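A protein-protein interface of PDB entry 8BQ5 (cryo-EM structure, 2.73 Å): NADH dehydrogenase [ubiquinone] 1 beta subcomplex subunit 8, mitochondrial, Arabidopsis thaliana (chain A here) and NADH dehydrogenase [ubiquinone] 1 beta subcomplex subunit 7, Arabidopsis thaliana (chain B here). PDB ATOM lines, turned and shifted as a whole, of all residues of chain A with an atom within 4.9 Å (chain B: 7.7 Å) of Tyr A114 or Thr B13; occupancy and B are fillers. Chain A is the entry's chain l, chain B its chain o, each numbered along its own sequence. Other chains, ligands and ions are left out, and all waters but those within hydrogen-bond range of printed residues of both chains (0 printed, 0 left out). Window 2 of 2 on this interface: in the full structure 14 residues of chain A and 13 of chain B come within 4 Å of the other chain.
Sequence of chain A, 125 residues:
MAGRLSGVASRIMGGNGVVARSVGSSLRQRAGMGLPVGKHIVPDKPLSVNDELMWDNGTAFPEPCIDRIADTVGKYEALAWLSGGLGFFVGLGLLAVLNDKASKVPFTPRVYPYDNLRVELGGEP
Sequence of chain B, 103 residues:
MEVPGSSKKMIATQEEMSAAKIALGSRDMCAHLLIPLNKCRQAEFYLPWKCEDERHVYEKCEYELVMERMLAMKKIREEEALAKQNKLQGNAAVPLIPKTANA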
ATOM      1  N   TYR A 112     -23.631  11.458  20.761  1.00  0.00           N
ATOM      2  CA  TYR A 112     -24.442  12.652  20.905  1.00  0.00           C
ATOM      3  C   TYR A 112     -23.746  13.864  20.292  1.00  0.00           C
ATOM      4  O   TYR A 112     -22.518  13.939  20.258  1.00  0.00           O
ATOM      5  CB  TYR A 112     -24.750  12.891  22.380  1.00  0.00           C
ATOM      6  CG  TYR A 112     -25.872  12.019  22.900  1.00  0.00           C
ATOM      7  CD1 TYR A 112     -25.651  10.686  23.222  1.00  0.00           C
ATOM      8  CD2 TYR A 112     -27.152  12.528  23.062  1.00  0.00           C
ATOM      9  CE1 TYR A 112     -26.678   9.885  23.692  1.00  0.00           C
ATOM     10  CE2 TYR A 112     -28.182  11.738  23.531  1.00  0.00           C
ATOM     11  CZ  TYR A 112     -27.941  10.420  23.844  1.00  0.00           C
ATOM     12  OH  TYR A 112     -28.968   9.635  24.311  1.00  0.00           O
ATOM     13  N   PRO A 113     -24.519  14.827  19.784  1.00  0.00           N
ATOM     14  CA  PRO A 113     -23.913  16.016  19.168  1.00  0.00           C
ATOM     15  C   PRO A 113     -23.270  16.957  20.174  1.00  0.00           C
ATOM     16  O   PRO A 113     -23.476  16.825  21.385  1.00  0.00           O
ATOM     17  CB  PRO A 113     -25.098  16.684  18.459  1.00  0.00           C
ATOM     18  CG  PRO A 113     -26.293  16.210  19.212  1.00  0.00           C
ATOM     19  CD  PRO A 113     -25.982  14.803  19.616  1.00  0.00           C
ATOM     20  N   TYR A 114     -22.495  17.917  19.665  1.00  0.00           N
ATOM     21  CA  TYR A 114     -21.754  18.880  20.482  1.00  0.00           C
ATOM     22  C   TYR A 114     -20.829  18.164  21.467  1.00  0.00           C
ATOM     23  O   TYR A 114     -20.975  18.261  22.687  1.00  0.00           O
ATOM     24  CB  TYR A 114     -22.703  19.843  21.202  1.00  0.00           C
ATOM     25  CG  TYR A 114     -23.674  20.527  20.272  1.00  0.00           C
ATOM     26  CD1 TYR A 114     -23.220  21.359  19.258  1.00  0.00           C
ATOM     27  CD2 TYR A 114     -25.042  20.344  20.407  1.00  0.00           C
ATOM     28  CE1 TYR A 114     -24.101  21.985  18.401  1.00  0.00           C
ATOM     29  CE2 TYR A 114     -25.933  20.966  19.555  1.00  0.00           C
ATOM     30  CZ  TYR A 114     -25.456  21.786  18.554  1.00  0.00           C
ATOM     31  OH  TYR A 114     -26.338  22.409  17.702  1.00  0.00           O
ATOM     32  N   ASP A 115     -19.869  17.432  20.901  1.00  0.00           N
ATOM     33  CA  ASP A 115     -18.833  16.740  21.668  1.00  0.00           C
ATOM     34  C   ASP A 115     -19.452  15.823  22.722  1.00  0.00           C
ATOM     35  O   ASP A 115     -19.039  15.803  23.885  1.00  0.00           O
ATOM     36  CB  ASP A 115     -17.864  17.744  22.301  1.00  0.00           C
ATOM     37  CG  ASP A 115     -16.537  17.114  22.690  1.00  0.00           C
ATOM     38  OD1 ASP A 115     -15.563  17.255  21.921  1.00  0.00           O
ATOM     39  OD2 ASP A 115     -16.460  16.488  23.766  1.00  0.00           O
ATOM     40  N   ASN A 116     -20.465  15.063  22.302  1.00  0.00           N
ATOM     41  CA  ASN A 116     -21.180  14.138  23.183  1.00  0.00           C
ATOM     42  C   ASN A 116     -21.702  14.848  24.430  1.00  0.00           C
ATOM     43  O   ASN A 116     -21.607  14.330  25.545  1.00  0.00           O
ATOM     44  CB  ASN A 116     -20.302  12.945  23.565  1.00  0.00           C
ATOM     45  CG  ASN A 116     -21.089  11.837  24.228  1.00  0.00           C
ATOM     46  OD1 ASN A 116     -22.270  11.640  23.936  1.00  0.00           O
ATOM     47  ND2 ASN A 116     -20.438  11.100  25.119  1.00  0.00           N
ATOM     48  N   LEU A 117     -22.251  16.045  24.232  1.00  0.00           N
ATOM     49  CA  LEU A 117     -22.815  16.857  25.309  1.00  0.00           C
ATOM     50  C   LEU A 117     -21.795  17.090  26.421  1.00  0.00           C
ATOM     51  O   LEU A 117     -22.070  16.881  27.603  1.00  0.00           O
ATOM     52  CB  LEU A 117     -24.094  16.225  25.857  1.00  0.00           C
ATOM     53  CG  LEU A 117     -25.192  15.944  24.834  1.00  0.00           C
ATOM     54  CD1 LEU A 117     -26.281  15.075  25.440  1.00  0.00           C
ATOM     55  CD2 LEU A 117     -25.769  17.250  24.322  1.00  0.00           C
ATOM     56  N   ARG A 118     -20.597  17.527  26.029  1.00  0.00           N
ATOM     57  CA  ARG A 118     -19.562  17.818  27.016  1.00  0.00           C
ATOM     58  C   ARG A 118     -19.941  19.015  27.880  1.00  0.00           C
ATOM     59  O   ARG A 118     -19.851  18.957  29.112  1.00  0.00           O
ATOM     60  CB  ARG A 118     -18.224  18.068  26.322  1.00  0.00           C
ATOM     61  CG  ARG A 118     -17.042  17.408  27.008  1.00  0.00           C
ATOM     62  CD  ARG A 118     -15.711  17.945  26.502  1.00  0.00           C
ATOM     63  NE  ARG A 118     -15.538  19.370  26.762  1.00  0.00           N
ATOM     64  CZ  ARG A 118     -15.756  20.330  25.873  1.00  0.00           C
ATOM     65  NH1 ARG A 118     -16.207  20.059  24.660  1.00  0.00           N
ATOM     66  NH2 ARG A 118     -15.516  21.593  26.211  1.00  0.00           N
ATOM     67  N   GLU A 120     -22.966  20.417  28.197  1.00  0.00           N
ATOM     68  CA  GLU A 120     -24.243  20.198  28.865  1.00  0.00           C
ATOM     69  C   GLU A 120     -24.130  19.224  30.028  1.00  0.00           C
ATOM     70  O   GLU A 120     -24.978  19.251  30.926  1.00  0.00           O
ATOM     71  CB  GLU A 120     -25.274  19.693  27.859  1.00  0.00           C
ATOM     72  CG  GLU A 120     -25.720  20.744  26.861  1.00  0.00           C
ATOM     73  CD  GLU A 120     -24.837  20.787  25.630  1.00  0.00           C
ATOM     74  OE1 GLU A 120     -23.629  20.497  25.749  1.00  0.00           O
ATOM     75  OE2 GLU A 120     -25.352  21.109  24.541  1.00  0.00           O
ATOM     76  N   MET B  10     -27.417  17.868  12.953  1.00  0.00           N
ATOM     77  CA  MET B  10     -28.019  18.626  14.042  1.00  0.00           C
ATOM     78  C   MET B  10     -28.731  19.860  13.503  1.00  0.00           C
ATOM     79  O   MET B  10     -28.144  20.663  12.771  1.00  0.00           O
ATOM     80  CB  MET B  10     -26.956  19.034  15.061  1.00  0.00           C
ATOM     81  CG  MET B  10     -27.457  19.072  16.500  1.00  0.00           C
ATOM     82  SD  MET B  10     -28.659  17.780  16.865  1.00  0.00           S
ATOM     83  CE  MET B  10     -29.200  18.263  18.501  1.00  0.00           C
ATOM     84  N   ILE B  11     -29.999  20.006  13.869  1.00  0.00           N
ATOM     85  CA  ILE B  11     -30.815  21.147  13.481  1.00  0.00           C
ATOM     86  C   ILE B  11     -31.110  22.042  14.677  1.00  0.00           C
ATOM     87  O   ILE B  11     -31.048  23.269  14.579  1.00  0.00           O
ATOM     88  CB  ILE B  11     -32.123  20.681  12.799  1.00  0.00           C
ATOM     89  CG1 ILE B  11     -31.819  20.075  11.429  1.00  0.00           C
ATOM     90  CG2 ILE B  11     -33.101  21.835  12.652  1.00  0.00           C
ATOM     91  CD1 ILE B  11     -32.762  18.966  11.027  1.00  0.00           C
ATOM     92  N   ALA B  12     -31.412  21.442  15.823  1.00  0.00           N
ATOM     93  CA  ALA B  12     -31.704  22.217  17.019  1.00  0.00           C
ATOM     94  C   ALA B  12     -30.411  22.587  17.731  1.00  0.00           C
ATOM     95  O   ALA B  12     -29.622  21.715  18.103  1.00  0.00           O
ATOM     96  CB  ALA B  12     -32.622  21.426  17.948  1.00  0.00           C
ATOM     97  N   THR B  13     -30.194  23.885  17.921  1.00  0.00           N
ATOM     98  CA  THR B  13     -28.979  24.368  18.554  1.00  0.00           C
ATOM     99  C   THR B  13     -29.021  24.119  20.060  1.00  0.00           C
ATOM    100  O   THR B  13     -30.038  23.716  20.626  1.00  0.00           O
ATOM    101  CB  THR B  13     -28.779  25.855  18.271  1.00  0.00           C
ATOM    102  OG1 THR B  13     -29.708  26.619  19.048  1.00  0.00           O
ATOM    103  CG2 THR B  13     -28.992  26.145  16.796  1.00  0.00           C
ATOM    104  N   GLN B  14     -27.883  24.375  20.711  1.00  0.00           N
ATOM    105  CA  GLN B  14     -27.780  24.146  22.148  1.00  0.00           C
ATOM    106  C   GLN B  14     -28.744  25.037  22.920  1.00  0.00           C
ATOM    107  O   GLN B  14     -29.366  24.594  23.893  1.00  0.00           O
ATOM    108  CB  GLN B  14     -26.349  24.391  22.618  1.00  0.00           C
ATOM    109  CG  GLN B  14     -25.389  23.261  22.325  1.00  0.00           C
ATOM    110  CD  GLN B  14     -23.957  23.736  22.218  1.00  0.00           C
ATOM    111  OE1 GLN B  14     -23.697  24.887  21.869  1.00  0.00           O
ATOM    112  NE2 GLN B  14     -23.017  22.856  22.533  1.00  0.00           N
ATOM    113  N   GLU B  15     -28.869  26.301  22.510  1.00  0.00           N
ATOM    114  CA  GLU B  15     -29.766  27.215  23.207  1.00  0.00           C
ATOM    115  C   GLU B  15     -31.212  26.755  23.083  1.00  0.00           C
ATOM    116  O   GLU B  15     -31.956  26.736  24.070  1.00  0.00           O
ATOM    117  CB  GLU B  15     -29.590  28.632  22.655  1.00  0.00           C
ATOM    118  CG  GLU B  15     -30.264  29.765  23.437  1.00  0.00           C
ATOM    119  CD  GLU B  15     -30.415  29.490  24.931  1.00  0.00           C
ATOM    120  OE1 GLU B  15     -31.344  28.767  25.332  1.00  0.00           O
ATOM    121  OE2 GLU B  15     -29.569  29.964  25.714  1.00  0.00           O
ATOM    122  N   GLU B  16     -31.619  26.337  21.885  1.00  0.00           N
ATOM    123  CA  GLU B  16     -33.003  25.918  21.687  1.00  0.00           C
ATOM    124  C   GLU B  16     -33.344  24.709  22.550  1.00  0.00           C
ATOM    125  O   GLU B  16     -34.430  24.643  23.138  1.00  0.00           O
ATOM    126  CB  GLU B  16     -33.247  25.619  20.211  1.00  0.00           C
ATOM    127  CG  GLU B  16     -33.021  26.809  19.297  1.00  0.00           C
ATOM    128  CD  GLU B  16     -34.206  27.755  19.276  1.00  0.00           C
ATOM    129  OE1 GLU B  16     -34.232  28.699  20.094  1.00  0.00           O
ATOM    130  OE2 GLU B  16     -35.117  27.549  18.448  1.00  0.00           O
ATOM    131  N   MET B  17     -32.442  23.728  22.602  1.00  0.00           N
ATOM    132  CA  MET B  17     -32.671  22.546  23.480  1.00  0.00           C
ATOM    133  C   MET B  17     -32.648  22.976  24.953  1.00  0.00           C
ATOM    134  O   MET B  17     -33.506  22.500  25.714  1.00  0.00           O
ATOM    135  CB  MET B  17     -31.606  21.478  23.246  1.00  0.00           C
ATOM    136  CG  MET B  17     -31.611  20.924  21.846  1.00  0.00           C
ATOM    137  SD  MET B  17     -30.349  19.651  21.664  1.00  0.00           S
ATOM    138  CE  MET B  17     -28.902  20.529  22.249  1.00  0.00           C
ATOM    139  N   SER B  18     -31.723  23.858  25.335  1.00  0.00           N
ATOM    140  CA  SER B  18     -31.665  24.378  26.728  1.00  0.00           C
ATOM    141  C   SER B  18     -32.937  25.167  27.055  1.00  0.00           C
ATOM    142  O   SER B  18     -33.405  25.071  28.196  1.00  0.00           O
ATOM    143  CB  SER B  18     -30.452  25.227  26.925  1.00  0.00           C
ATOM    144  OG  SER B  18     -29.267  24.479  26.710  1.00  0.00           O
ATOM    145  N   ALA B  19     -33.486  25.900  26.082  1.00  0.00           N
ATOM    146  CA  ALA B  19     -34.694  26.727  26.312  1.00  0.00           C
ATOM    147  C   ALA B  19     -35.919  25.826  26.462  1.00  0.00           C
ATOM    148  O   ALA B  19     -36.794  26.166  27.271  1.00  0.00           O
ATOM    149  CB  ALA B  19     -34.863  27.719  25.189  1.00  0.00           C
ATOM    150  N   ARG B  27     -31.157  14.864  23.835  1.00  0.00           N
ATOM    151  CA  ARG B  27     -30.496  15.864  22.961  1.00  0.00           C
ATOM    152  C   ARG B  27     -29.803  15.097  21.831  1.00  0.00           C
ATOM    153  O   ARG B  27     -28.589  15.265  21.666  1.00  0.00           O
ATOM    154  CB  ARG B  27     -29.551  16.723  23.807  1.00  0.00           C
ATOM    155  CG  ARG B  27     -30.164  17.227  25.107  1.00  0.00           C
ATOM    156  CD  ARG B  27     -29.613  18.544  25.618  1.00  0.00           C
ATOM    157  NE  ARG B  27     -30.629  19.271  26.365  1.00  0.00           N
ATOM    158  CZ  ARG B  27     -30.434  20.395  27.046  1.00  0.00           C
ATOM    159  NH1 ARG B  27     -29.239  20.957  27.091  1.00  0.00           N
ATOM    160  NH2 ARG B  27     -31.442  20.957  27.686  1.00  0.00           N
ATOM    161  N   ASP B  28     -30.552  14.269  21.098  1.00  0.00           N
ATOM    162  CA  ASP B  28     -29.995  13.425  20.004  1.00  0.00           C
ATOM    163  C   ASP B  28     -29.984  14.202  18.685  1.00  0.00           C
ATOM    164  O   ASP B  28     -29.505  15.327  18.686  1.00  0.00           O
ATOM    165  CB  ASP B  28     -30.785  12.120  19.875  1.00  0.00           C
ATOM    166  CG  ASP B  28     -32.253  12.315  19.536  1.00  0.00           C
ATOM    167  OD1 ASP B  28     -32.694  13.478  19.472  1.00  0.00           O
ATOM    168  OD2 ASP B  28     -32.945  11.299  19.355  1.00  0.00           O
ATOM    169  N   MET B  29     -30.460  13.592  17.599  1.00  0.00           N
ATOM    170  CA  MET B  29     -30.536  14.285  16.286  1.00  0.00           C
ATOM    171  C   MET B  29     -31.994  14.649  15.998  1.00  0.00           C
ATOM    172  O   MET B  29     -32.231  15.434  15.063  1.00  0.00           O
ATOM    173  CB  MET B  29     -29.997  13.405  15.154  1.00  0.00           C
ATOM    174  CG  MET B  29     -28.488  13.250  15.175  1.00  0.00           C
ATOM    175  SD  MET B  29     -27.653  14.579  14.271  1.00  0.00           S
ATOM    176  CE  MET B  29     -25.997  14.447  14.939  1.00  0.00           C
ATOM    177  N   ALA B  31     -33.869  16.213  18.265  1.00  0.00           N
ATOM    178  CA  ALA B  31     -34.257  17.227  19.263  1.00  0.00           C
ATOM    179  C   ALA B  31     -35.211  18.238  18.626  1.00  0.00           C
ATOM    180  O   ALA B  31     -36.087  18.751  19.351  1.00  0.00           O
ATOM    181  CB  ALA B  31     -33.018  17.891  19.765  1.00  0.00           C
ATOM    182  N   HIS B  32     -35.051  18.513  17.326  1.00  0.00           N
ATOM    183  CA  HIS B  32     -35.887  19.541  16.641  1.00  0.00           C
ATOM    184  C   HIS B  32     -37.356  19.111  16.618  1.00  0.00           C
ATOM    185  O   HIS B  32     -38.213  19.994  16.723  1.00  0.00           O
ATOM    186  CB  HIS B  32     -35.346  19.849  15.235  1.00  0.00           C
ATOM    187  CG  HIS B  32     -35.359  18.690  14.296  1.00  0.00           C
ATOM    188  ND1 HIS B  32     -34.565  17.575  14.482  1.00  0.00           N
ATOM    189  CD2 HIS B  32     -36.046  18.478  13.153  1.00  0.00           C
ATOM    190  CE1 HIS B  32     -34.777  16.719  13.505  1.00  0.00           C
ATOM    191  NE2 HIS B  32     -35.679  17.250  12.676  1.00  0.00           N
ATOM    192  N   ILE B  35     -39.265  19.323  20.418  1.00  0.00           N
ATOM    193  CA  ILE B  35     -39.754  20.595  20.954  1.00  0.00           C
ATOM    194  C   ILE B  35     -41.228  20.831  20.641  1.00  0.00           C
ATOM    195  O   ILE B  35     -41.983  21.180  21.563  1.00  0.00           O
ATOM    196  CB  ILE B  35     -38.854  21.749  20.475  1.00  0.00           C
ATOM    197  CG1 ILE B  35     -37.441  21.591  21.031  1.00  0.00           C
ATOM    198  CG2 ILE B  35     -39.434  23.091  20.891  1.00  0.00           C
ATOM    199  CD1 ILE B  35     -36.528  22.739  20.689  1.00  0.00           C
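Of the printed residues of chain B, Tyr A112 touches Arg B27 (3.4 Å). Tyr A114 touches just these residues of chain B: Met B10, Ala B12, Thr B13 and Gln B14. Asp A115 touches none of the printed residues of chain B. Printed residues of chain B within 4 Å of Glu A120: Gln B14 and Arg B27. Of the printed residues of chain A, Met B10 touches Pro A113 and Tyr A114. Of the printed residues of chain A, Ala B12 touches Tyr A114. Printed residues of chain A within 4 Å of Asp B28: Pro A113 (3.4 Å). Ile B35 touches none of the printed residues of chain A.
Printed residues of chain B that touch a printed residue of chain A: Met B10, Ala B12, Thr B13, Gln B14, Arg B27 and Asp B28. Hydrophobic or aromatic side chains of chain B that line the printed part of chain A: Met B10. Of the 8 printed residues of chain A, 5 touch a printed residue of chain B. Printed residues of chain A that touch a printed residue of chain B: Tyr A112, Pro A113, Tyr A114, Leu A117 and Glu A120. Among the printed residues, 11 pairs touch across the chains. Among the printed residues, no Asp or Glu carboxylate lies within 4 Å of a Lys or Arg side-chain nitrogen of the other chain.
The backbone carbonyl oxygen of Ala B12 lies within hydrogen-bond range of the side-chain hydroxyl of Tyr A114 (3.4 Å).
The side-chain amide oxygen (OD1) of Asn A116 sits close to the backbone NH (N) of Tyr A112, at 3.5 Å. SD of Met B29 sits at hydrogen-bond distance from N of Met B10. The backbone NH of Glu B16 lies close to the side-chain hydroxyl of Thr B13 (3.4 Å). The side-chain hydroxyl (OG) of Ser B18 lies within hydrogen-bond range of the backbone carbonyl oxygen (O) of Gln B14 (2.8 Å). The backbone carbonyl oxygen (O) of Met B17 is in hydrogen-bond range of the guanidinium group (NH2) of Arg B27 (3.2 Å). The side-chain carboxylate of Asp B28 sits at hydrogen-bond distance from the backbone NH of Ala B31, at 3.2 Å.
Among the printed residues, merely in contact across the chains: Glu A120 with Gln B14, Tyr A114 with Gln B14, Pro A113 with Arg B27, Pro A113 with Asp B28, Tyr A112 with Arg B27, Tyr A114 with Thr B13, Glu A120 with Arg B27, Pro A113 with Met B10, Tyr A114 with Met B10 and Leu A117 with Arg B27.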
